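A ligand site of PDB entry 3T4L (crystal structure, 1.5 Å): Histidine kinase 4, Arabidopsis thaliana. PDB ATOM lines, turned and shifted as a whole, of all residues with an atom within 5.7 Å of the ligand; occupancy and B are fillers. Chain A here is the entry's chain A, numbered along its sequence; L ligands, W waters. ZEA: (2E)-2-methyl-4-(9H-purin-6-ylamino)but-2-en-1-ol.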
ATOM      1  N   SER A  74       9.785 -24.659  28.525  1.00  0.00           N
ATOM      2  CA  SER A  74      10.955 -25.516  28.589  1.00  0.00           C
ATOM      3  C   SER A  74      12.025 -24.918  29.503  1.00  0.00           C
ATOM      4  O   SER A  74      12.832 -25.644  30.075  1.00  0.00           O
ATOM      5  CB  SER A  74      11.536 -25.758  27.197  1.00  0.00           C
ATOM      6  OG  SER A  74      11.929 -24.575  26.564  1.00  0.00           O
ATOM      7  N   GLY A  75      12.037 -23.591  29.640  1.00  0.00           N
ATOM      8  CA  GLY A  75      13.034 -22.919  30.464  1.00  0.00           C
ATOM      9  C   GLY A  75      12.743 -21.430  30.505  1.00  0.00           C
ATOM     10  O   GLY A  75      12.000 -20.914  29.682  1.00  0.00           O
ATOM     11  N   ALA A  77      14.851 -17.536  31.565  1.00  0.00           N
ATOM     12  CA  ALA A  77      16.150 -16.904  31.646  1.00  0.00           C
ATOM     13  C   ALA A  77      15.936 -15.399  31.826  1.00  0.00           C
ATOM     14  O   ALA A  77      14.913 -14.849  31.428  1.00  0.00           O
ATOM     15  CB  ALA A  77      16.968 -17.156  30.389  1.00  0.00           C
ATOM     16  N   TYR A  78      16.949 -14.749  32.356  1.00  0.00           N
ATOM     17  CA  TYR A  78      16.975 -13.289  32.500  1.00  0.00           C
ATOM     18  C   TYR A  78      18.142 -12.705  31.705  1.00  0.00           C
ATOM     19  O   TYR A  78      19.296 -13.066  31.917  1.00  0.00           O
ATOM     20  CB  TYR A  78      17.112 -12.864  33.963  1.00  0.00           C
ATOM     21  CG  TYR A  78      17.136 -11.381  34.086  1.00  0.00           C
ATOM     22  CD1 TYR A  78      16.008 -10.614  33.774  1.00  0.00           C
ATOM     23  CD2 TYR A  78      18.298 -10.710  34.444  1.00  0.00           C
ATOM     24  CE1 TYR A  78      16.031  -9.226  33.832  1.00  0.00           C
ATOM     25  CE2 TYR A  78      18.322  -9.304  34.502  1.00  0.00           C
ATOM     26  CZ  TYR A  78      17.193  -8.589  34.192  1.00  0.00           C
ATOM     27  OH  TYR A  78      17.238  -7.196  34.221  1.00  0.00           O
ATOM     28  N   ALA A  79      17.791 -11.782  30.796  1.00  0.00           N
ATOM     29  CA  ALA A  79      18.765 -11.081  29.961  1.00  0.00           C
ATOM     30  C   ALA A  79      18.829  -9.646  30.442  1.00  0.00           C
ATOM     31  O   ALA A  79      17.815  -9.031  30.670  1.00  0.00           O
ATOM     32  CB  ALA A  79      18.341 -11.122  28.494  1.00  0.00           C
ATOM     33  N   MET A 101      23.710 -15.472  18.958  1.00  0.00           N
ATOM     34  CA  MET A 101      22.864 -16.647  19.071  1.00  0.00           C
ATOM     35  C   MET A 101      23.108 -17.650  17.959  1.00  0.00           C
ATOM     36  O   MET A 101      22.987 -18.861  18.170  1.00  0.00           O
ATOM     37  CB  MET A 101      21.432 -16.152  18.971  1.00  0.00           C
ATOM     38  CG  MET A 101      20.396 -17.122  19.093  1.00  0.00           C
ATOM     39  SD  MET A 101      18.944 -16.173  18.742  1.00  0.00           S
ATOM     40  CE  MET A 101      18.991 -15.004  20.109  1.00  0.00           C
ATOM     41  N   VAL A 116      22.093 -12.988  28.225  1.00  0.00           N
ATOM     42  CA  VAL A 116      21.486 -13.738  29.297  1.00  0.00           C
ATOM     43  C   VAL A 116      22.527 -13.890  30.410  1.00  0.00           C
ATOM     44  O   VAL A 116      23.659 -14.368  30.180  1.00  0.00           O
ATOM     45  CB  VAL A 116      21.050 -15.087  28.824  1.00  0.00           C
ATOM     46  CG1 VAL A 116      20.727 -16.009  30.043  1.00  0.00           C
ATOM     47  CG2 VAL A 116      19.816 -14.954  27.948  1.00  0.00           C
ATOM     48  N   VAL A 123      17.877 -24.431  29.977  1.00  0.00           N
ATOM     49  CA  VAL A 123      18.275 -23.570  28.869  1.00  0.00           C
ATOM     50  C   VAL A 123      19.613 -22.897  29.159  1.00  0.00           C
ATOM     51  O   VAL A 123      19.832 -21.730  28.868  1.00  0.00           O
ATOM     52  CB  VAL A 123      17.198 -22.520  28.564  1.00  0.00           C
ATOM     53  CG1 VAL A 123      15.981 -23.199  27.942  1.00  0.00           C
ATOM     54  CG2 VAL A 123      16.822 -21.702  29.803  1.00  0.00           C
ATOM     55  N   TYR A 125      22.481 -23.231  27.824  1.00  0.00           N
ATOM     56  CA  TYR A 125      23.137 -22.798  26.598  1.00  0.00           C
ATOM     57  C   TYR A 125      22.821 -21.350  26.211  1.00  0.00           C
ATOM     58  O   TYR A 125      23.498 -20.796  25.367  1.00  0.00           O
ATOM     59  CB  TYR A 125      22.778 -23.720  25.424  1.00  0.00           C
ATOM     60  CG  TYR A 125      21.299 -24.004  25.314  1.00  0.00           C
ATOM     61  CD1 TYR A 125      20.437 -23.099  24.703  1.00  0.00           C
ATOM     62  CD2 TYR A 125      20.762 -25.177  25.822  1.00  0.00           C
ATOM     63  CE1 TYR A 125      19.076 -23.362  24.587  1.00  0.00           C
ATOM     64  CE2 TYR A 125      19.405 -25.440  25.719  1.00  0.00           C
ATOM     65  CZ  TYR A 125      18.574 -24.541  25.098  1.00  0.00           C
ATOM     66  OH  TYR A 125      17.239 -24.838  25.027  1.00  0.00           O
ATOM     67  N   LEU A 126      21.805 -20.746  26.824  1.00  0.00           N
ATOM     68  CA  LEU A 126      21.526 -19.323  26.589  1.00  0.00           C
ATOM     69  C   LEU A 126      22.527 -18.396  27.278  1.00  0.00           C
ATOM     70  O   LEU A 126      22.636 -17.243  26.866  1.00  0.00           O
ATOM     71  CB  LEU A 126      20.127 -18.931  27.066  1.00  0.00           C
ATOM     72  CG  LEU A 126      18.911 -19.577  26.405  1.00  0.00           C
ATOM     73  CD1 LEU A 126      17.632 -19.116  27.117  1.00  0.00           C
ATOM     74  CD2 LEU A 126      18.861 -19.236  24.902  1.00  0.00           C
ATOM     75  N   MET A 131      20.288 -11.889  23.281  1.00  0.00           N
ATOM     76  CA  MET A 131      18.963 -12.251  22.787  1.00  0.00           C
ATOM     77  C   MET A 131      18.488 -11.285  21.692  1.00  0.00           C
ATOM     78  O   MET A 131      17.560 -11.596  20.957  1.00  0.00           O
ATOM     79  CB  MET A 131      17.970 -12.421  23.939  1.00  0.00           C
ATOM     80  CG  MET A 131      18.395 -13.509  24.963  1.00  0.00           C
ATOM     81  SD  MET A 131      18.965 -15.059  24.246  1.00  0.00           S
ATOM     82  CE  MET A 131      17.497 -15.665  23.455  1.00  0.00           C
ATOM     83  N   ASP A 137      13.386 -12.860  18.889  1.00  0.00           N
ATOM     84  CA  ASP A 137      13.736 -12.418  20.241  1.00  0.00           C
ATOM     85  C   ASP A 137      13.922 -10.909  20.358  1.00  0.00           C
ATOM     86  O   ASP A 137      13.468 -10.294  21.331  1.00  0.00           O
ATOM     87  CB  ASP A 137      14.968 -13.152  20.735  1.00  0.00           C
ATOM     88  CG  ASP A 137      14.650 -14.554  21.226  1.00  0.00           C
ATOM     89  OD1 ASP A 137      14.167 -14.615  22.374  1.00  0.00           O
ATOM     90  OD2 ASP A 137      14.932 -15.528  20.486  1.00  0.00           O
ATOM     91  N   ASN A 140      10.601  -9.124  20.231  1.00  0.00           N
ATOM     92  CA  ASN A 140       9.929  -9.359  21.501  1.00  0.00           C
ATOM     93  C   ASN A 140      10.457  -8.459  22.602  1.00  0.00           C
ATOM     94  O   ASN A 140       9.712  -7.831  23.331  1.00  0.00           O
ATOM     95  CB  ASN A 140      10.045 -10.838  21.905  1.00  0.00           C
ATOM     96  CG  ASN A 140       8.722 -11.450  22.275  1.00  0.00           C
ATOM     97  OD1 ASN A 140       7.709 -11.220  21.640  1.00  0.00           O
ATOM     98  ND2 ASN A 140       8.741 -12.272  23.335  1.00  0.00           N
ATOM     99  N   ILE A 141      11.776  -8.318  22.675  1.00  0.00           N
ATOM    100  CA  ILE A 141      12.423  -7.458  23.666  1.00  0.00           C
ATOM    101  C   ILE A 141      11.978  -6.018  23.527  1.00  0.00           C
ATOM    102  O   ILE A 141      11.590  -5.370  24.501  1.00  0.00           O
ATOM    103  CB  ILE A 141      13.938  -7.642  23.578  1.00  0.00           C
ATOM    104  CG1 ILE A 141      14.296  -8.947  24.317  1.00  0.00           C
ATOM    105  CG2 ILE A 141      14.729  -6.430  24.079  1.00  0.00           C
ATOM    106  CD1 ILE A 141      15.729  -9.482  24.071  1.00  0.00           C
ATOM    107  N   PHE A 156       8.463 -20.012  15.886  1.00  0.00           N
ATOM    108  CA  PHE A 156       9.767 -20.258  15.227  1.00  0.00           C
ATOM    109  C   PHE A 156      10.522 -21.384  15.922  1.00  0.00           C
ATOM    110  O   PHE A 156      10.149 -21.789  17.024  1.00  0.00           O
ATOM    111  CB  PHE A 156      10.619 -18.971  15.153  1.00  0.00           C
ATOM    112  CG  PHE A 156      11.183 -18.522  16.463  1.00  0.00           C
ATOM    113  CD1 PHE A 156      10.385 -17.915  17.423  1.00  0.00           C
ATOM    114  CD2 PHE A 156      12.539 -18.653  16.717  1.00  0.00           C
ATOM    115  CE1 PHE A 156      10.909 -17.509  18.620  1.00  0.00           C
ATOM    116  CE2 PHE A 156      13.058 -18.218  17.907  1.00  0.00           C
ATOM    117  CZ  PHE A 156      12.257 -17.641  18.847  1.00  0.00           C
ATOM    118  N   ARG A 157      11.570 -21.880  15.267  1.00  0.00           N
ATOM    119  CA  ARG A 157      12.322 -23.005  15.815  1.00  0.00           C
ATOM    120  C   ARG A 157      13.374 -22.509  16.803  1.00  0.00           C
ATOM    121  O   ARG A 157      14.244 -21.674  16.514  1.00  0.00           O
ATOM    122  CB  ARG A 157      12.911 -23.902  14.719  1.00  0.00           C
ATOM    123  CG  ARG A 157      11.820 -24.725  14.018  1.00  0.00           C
ATOM    124  CD  ARG A 157      12.295 -25.817  13.096  1.00  0.00           C
ATOM    125  NE  ARG A 157      11.135 -26.530  12.539  1.00  0.00           N
ATOM    126  CZ  ARG A 157      10.402 -27.448  13.173  1.00  0.00           C
ATOM    127  NH1 ARG A 157      10.695 -27.846  14.411  1.00  0.00           N
ATOM    128  NH2 ARG A 157       9.353 -27.991  12.547  1.00  0.00           N
ATOM    129  N   LEU A 158      13.243 -23.012  18.019  1.00  0.00           N
ATOM    130  CA  LEU A 158      14.005 -22.564  19.164  1.00  0.00           C
ATOM    131  C   LEU A 158      15.439 -23.082  19.102  1.00  0.00           C
ATOM    132  O   LEU A 158      15.774 -24.066  18.441  1.00  0.00           O
ATOM    133  CB  LEU A 158      13.326 -23.035  20.457  1.00  0.00           C
ATOM    134  CG  LEU A 158      11.891 -22.547  20.684  1.00  0.00           C
ATOM    135  CD1 LEU A 158      11.305 -23.204  21.946  1.00  0.00           C
ATOM    136  CD2 LEU A 158      11.797 -21.012  20.752  1.00  0.00           C
ATOM    137  N   LEU A 159      16.316 -22.390  19.813  1.00  0.00           N
ATOM    138  CA  LEU A 159      17.715 -22.757  19.905  1.00  0.00           C
ATOM    139  C   LEU A 159      17.898 -24.134  20.493  1.00  0.00           C
ATOM    140  O   LEU A 159      17.145 -24.542  21.356  1.00  0.00           O
ATOM    141  CB  LEU A 159      18.459 -21.751  20.796  1.00  0.00           C
ATOM    142  CG  LEU A 159      18.748 -20.395  20.146  1.00  0.00           C
ATOM    143  CD1 LEU A 159      19.250 -19.455  21.231  1.00  0.00           C
ATOM    144  CD2 LEU A 159      19.734 -20.497  18.981  1.00  0.00           C
ATOM    145  N   VAL A 167       8.349 -17.565  22.039  1.00  0.00           N
ATOM    146  CA  VAL A 167       9.016 -16.971  23.187  1.00  0.00           C
ATOM    147  C   VAL A 167       8.130 -15.928  23.844  1.00  0.00           C
ATOM    148  O   VAL A 167       7.477 -15.121  23.141  1.00  0.00           O
ATOM    149  CB  VAL A 167      10.373 -16.406  22.793  1.00  0.00           C
ATOM    150  CG1 VAL A 167      10.940 -15.502  23.882  1.00  0.00           C
ATOM    151  CG2 VAL A 167      11.332 -17.560  22.509  1.00  0.00           C
ATOM    152  N   LEU A 168       8.121 -15.944  25.171  1.00  0.00           N
ATOM    153  CA  LEU A 168       7.398 -14.990  26.003  1.00  0.00           C
ATOM    154  C   LEU A 168       8.441 -14.110  26.695  1.00  0.00           C
ATOM    155  O   LEU A 168       9.417 -14.620  27.231  1.00  0.00           O
ATOM    156  CB  LEU A 168       6.596 -15.737  27.067  1.00  0.00           C
ATOM    157  CG  LEU A 168       6.090 -14.942  28.273  1.00  0.00           C
ATOM    158  CD1 LEU A 168       4.884 -14.066  27.894  1.00  0.00           C
ATOM    159  CD2 LEU A 168       5.672 -15.865  29.433  1.00  0.00           C
ATOM    160  N   THR A 169       8.206 -12.789  26.709  1.00  0.00           N
ATOM    161  CA  THR A 169       9.118 -11.850  27.373  1.00  0.00           C
ATOM    162  C   THR A 169       8.345 -10.854  28.233  1.00  0.00           C
ATOM    163  O   THR A 169       7.274 -10.379  27.823  1.00  0.00           O
ATOM    164  CB  THR A 169       9.946 -11.091  26.322  1.00  0.00           C
ATOM    165  OG1 THR A 169      10.653 -12.033  25.495  1.00  0.00           O
ATOM    166  CG2 THR A 169      10.937 -10.129  27.021  1.00  0.00           C
ATOM    167  N   TYR A 193      15.116  -8.254  30.720  1.00  0.00           N
ATOM    168  CA  TYR A 193      14.031  -8.959  30.088  1.00  0.00           C
ATOM    169  C   TYR A 193      13.995 -10.373  30.648  1.00  0.00           C
ATOM    170  O   TYR A 193      14.977 -11.093  30.589  1.00  0.00           O
ATOM    171  CB  TYR A 193      14.268  -8.992  28.559  1.00  0.00           C
ATOM    172  CG  TYR A 193      14.838  -7.694  28.009  1.00  0.00           C
ATOM    173  CD1 TYR A 193      14.007  -6.591  27.833  1.00  0.00           C
ATOM    174  CD2 TYR A 193      16.173  -7.564  27.759  1.00  0.00           C
ATOM    175  CE1 TYR A 193      14.516  -5.393  27.386  1.00  0.00           C
ATOM    176  CE2 TYR A 193      16.705  -6.372  27.312  1.00  0.00           C
ATOM    177  CZ  TYR A 193      15.857  -5.298  27.113  1.00  0.00           C
ATOM    178  OH  TYR A 193      16.425  -4.113  26.633  1.00  0.00           O
ATOM    179  N   LEU A 194      12.843 -10.745  31.196  1.00  0.00           N
ATOM    180  CA  LEU A 194      12.636 -12.096  31.710  1.00  0.00           C
ATOM    181  C   LEU A 194      11.906 -12.871  30.608  1.00  0.00           C
ATOM    182  O   LEU A 194      10.801 -12.517  30.220  1.00  0.00           O
ATOM    183  CB  LEU A 194      11.827 -12.067  33.015  1.00  0.00           C
ATOM    184  CG  LEU A 194      11.958 -13.294  33.925  1.00  0.00           C
ATOM    185  CD1 LEU A 194      11.635 -14.612  33.217  1.00  0.00           C
ATOM    186  CD2 LEU A 194      13.378 -13.393  34.500  1.00  0.00           C
ATOM    187  N   GLY A 195      12.567 -13.902  30.079  1.00  0.00           N
ATOM    188  CA  GLY A 195      12.019 -14.675  28.973  1.00  0.00           C
ATOM    189  C   GLY A 195      11.744 -16.116  29.312  1.00  0.00           C
ATOM    190  O   GLY A 195      12.406 -16.716  30.168  1.00  0.00           O
ATOM    191  N   GLY A 196      10.787 -16.675  28.599  1.00  0.00           N
ATOM    192  CA  GLY A 196      10.423 -18.070  28.726  1.00  0.00           C
ATOM    193  C   GLY A 196      10.200 -18.641  27.353  1.00  0.00           C
ATOM    194  O   GLY A 196       9.640 -17.973  26.492  1.00  0.00           O
ATOM    195  N   ALA A 197      10.647 -19.884  27.147  1.00  0.00           N
ATOM    196  CA  ALA A 197      10.448 -20.597  25.880  1.00  0.00           C
ATOM    197  C   ALA A 197       9.235 -21.542  25.989  1.00  0.00           C
ATOM    198  O   ALA A 197       9.286 -22.530  26.748  1.00  0.00           O
ATOM    199  CB  ALA A 197      11.678 -21.403  25.563  1.00  0.00           C
HETATM  200  O16 ZEA L   1      13.303 -12.122  26.180  1.00  0.00           O
HETATM  201  C14 ZEA L   1      14.401 -12.564  26.914  1.00  0.00           C
HETATM  202  C13 ZEA L   1      14.768 -14.021  26.827  1.00  0.00           C
HETATM  203  C15 ZEA L   1      15.725 -14.539  27.857  1.00  0.00           C
HETATM  204  C12 ZEA L   1      14.063 -14.819  25.962  1.00  0.00           C
HETATM  205  C11 ZEA L   1      14.205 -16.302  25.878  1.00  0.00           C
HETATM  206  N10 ZEA L   1      14.358 -16.723  24.511  1.00  0.00           N
HETATM  207  C6  ZEA L   1      14.666 -18.094  24.210  1.00  0.00           C
HETATM  208  C5  ZEA L   1      14.918 -18.520  22.887  1.00  0.00           C
HETATM  209  N9  ZEA L   1      14.976 -17.901  21.646  1.00  0.00           N
HETATM  210  C4  ZEA L   1      15.226 -19.859  22.681  1.00  0.00           C
HETATM  211  N7  ZEA L   1      15.431 -20.042  21.351  1.00  0.00           N
HETATM  212  C8  ZEA L   1      15.339 -18.841  20.740  1.00  0.00           C
HETATM  213  N3  ZEA L   1      15.142 -20.749  23.745  1.00  0.00           N
HETATM  214  C2  ZEA L   1      14.935 -20.280  24.972  1.00  0.00           C
HETATM  215  N1  ZEA L   1      14.656 -18.992  25.236  1.00  0.00           N
HETATM  216  O   HOH W   1      14.174 -19.051  28.108  1.00  0.00           O
HETATM  217  O   HOH W   2      13.648 -12.319  23.521  1.00  0.00           O
HETATM  218  O   HOH W   3      15.660 -23.400  23.414  1.00  0.00           O
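A nitrogen (N9) of the ligand lies within hydrogen-bond range of the side-chain carboxylate (OD2) of Asp 137, at 2.6 Å. The side-chain hydroxyl of Thr 169 lies within hydrogen-bond range of an oxygen (O16) of the ligand (2.7 Å). N of Leu 159 sits close to N7 of the ligand (2.9 Å).
The side-chain hydroxyl (OG1) of Thr 169 sits at hydrogen-bond distance from the side-chain amide nitrogen (ND2) of Asn 140 (2.9 Å). The backbone carbonyl oxygen (O) of Ala 197 sits at hydrogen-bond distance from the backbone NH (N) of Ser 74 (2.8 Å). N of Ala 197 lies within hydrogen-bond range of O of Gly 75. N of Gly 195 is in hydrogen-bond range of O of Ala 77, at 2.9 Å. The backbone carbonyl oxygen (O) of Val 167 sits at hydrogen-bond distance from the side-chain amide nitrogen (ND2) of Asn 140 (3.1 Å). N of Tyr 193 is in hydrogen-bond range of O of Ala 79 (2.8 Å).
Merely in contact with the ligand: Ala 77 (3.7 Å), Leu 126 (3.5 Å), Met 131 (3.5 Å), Ile 141 (3.8 Å), Phe 156 (3.7 Å), Leu 158 (3.6 Å), Val 167 (3.7 Å), Tyr 193 (3.9 Å), Gly 195 (3.5 Å) and Ala 197 (3.5 Å). Hydrophobic or aromatic side chains within 4 Å of the ligand: Ala 77, Leu 126, Met 131, Ile 141, Phe 156, Leu 158, Leu 159, Val 167, Tyr 193 and Ala 197. Within 4 Å of the ligand: Ala 77, Leu 126, Met 131, Asp 137, Ile 141, Phe 156, Leu 158, Leu 159, Val 167, Thr 169, Tyr 193, Gly 195 and Ala 197. The nearest printed residue that does not touch the ligand is Val 116 (4.1 Å).
Water W2 lies within hydrogen-bond range of the side-chain carboxylate (OD1) of Asp 137 (2.6 Å) and an oxygen (O16) of the ligand (2.7 Å). Water W3 lies within hydrogen-bond range of the side-chain hydroxyl (OH) of Tyr 125 (2.7 Å), a nitrogen (N3) of the ligand (2.7 Å) and the backbone carbonyl oxygen (O) of Leu 159 (2.8 Å). Water W1 lies within hydrogen-bond range of N1 of the ligand (2.9 Å) and O of Gly 75 (3.3 Å).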
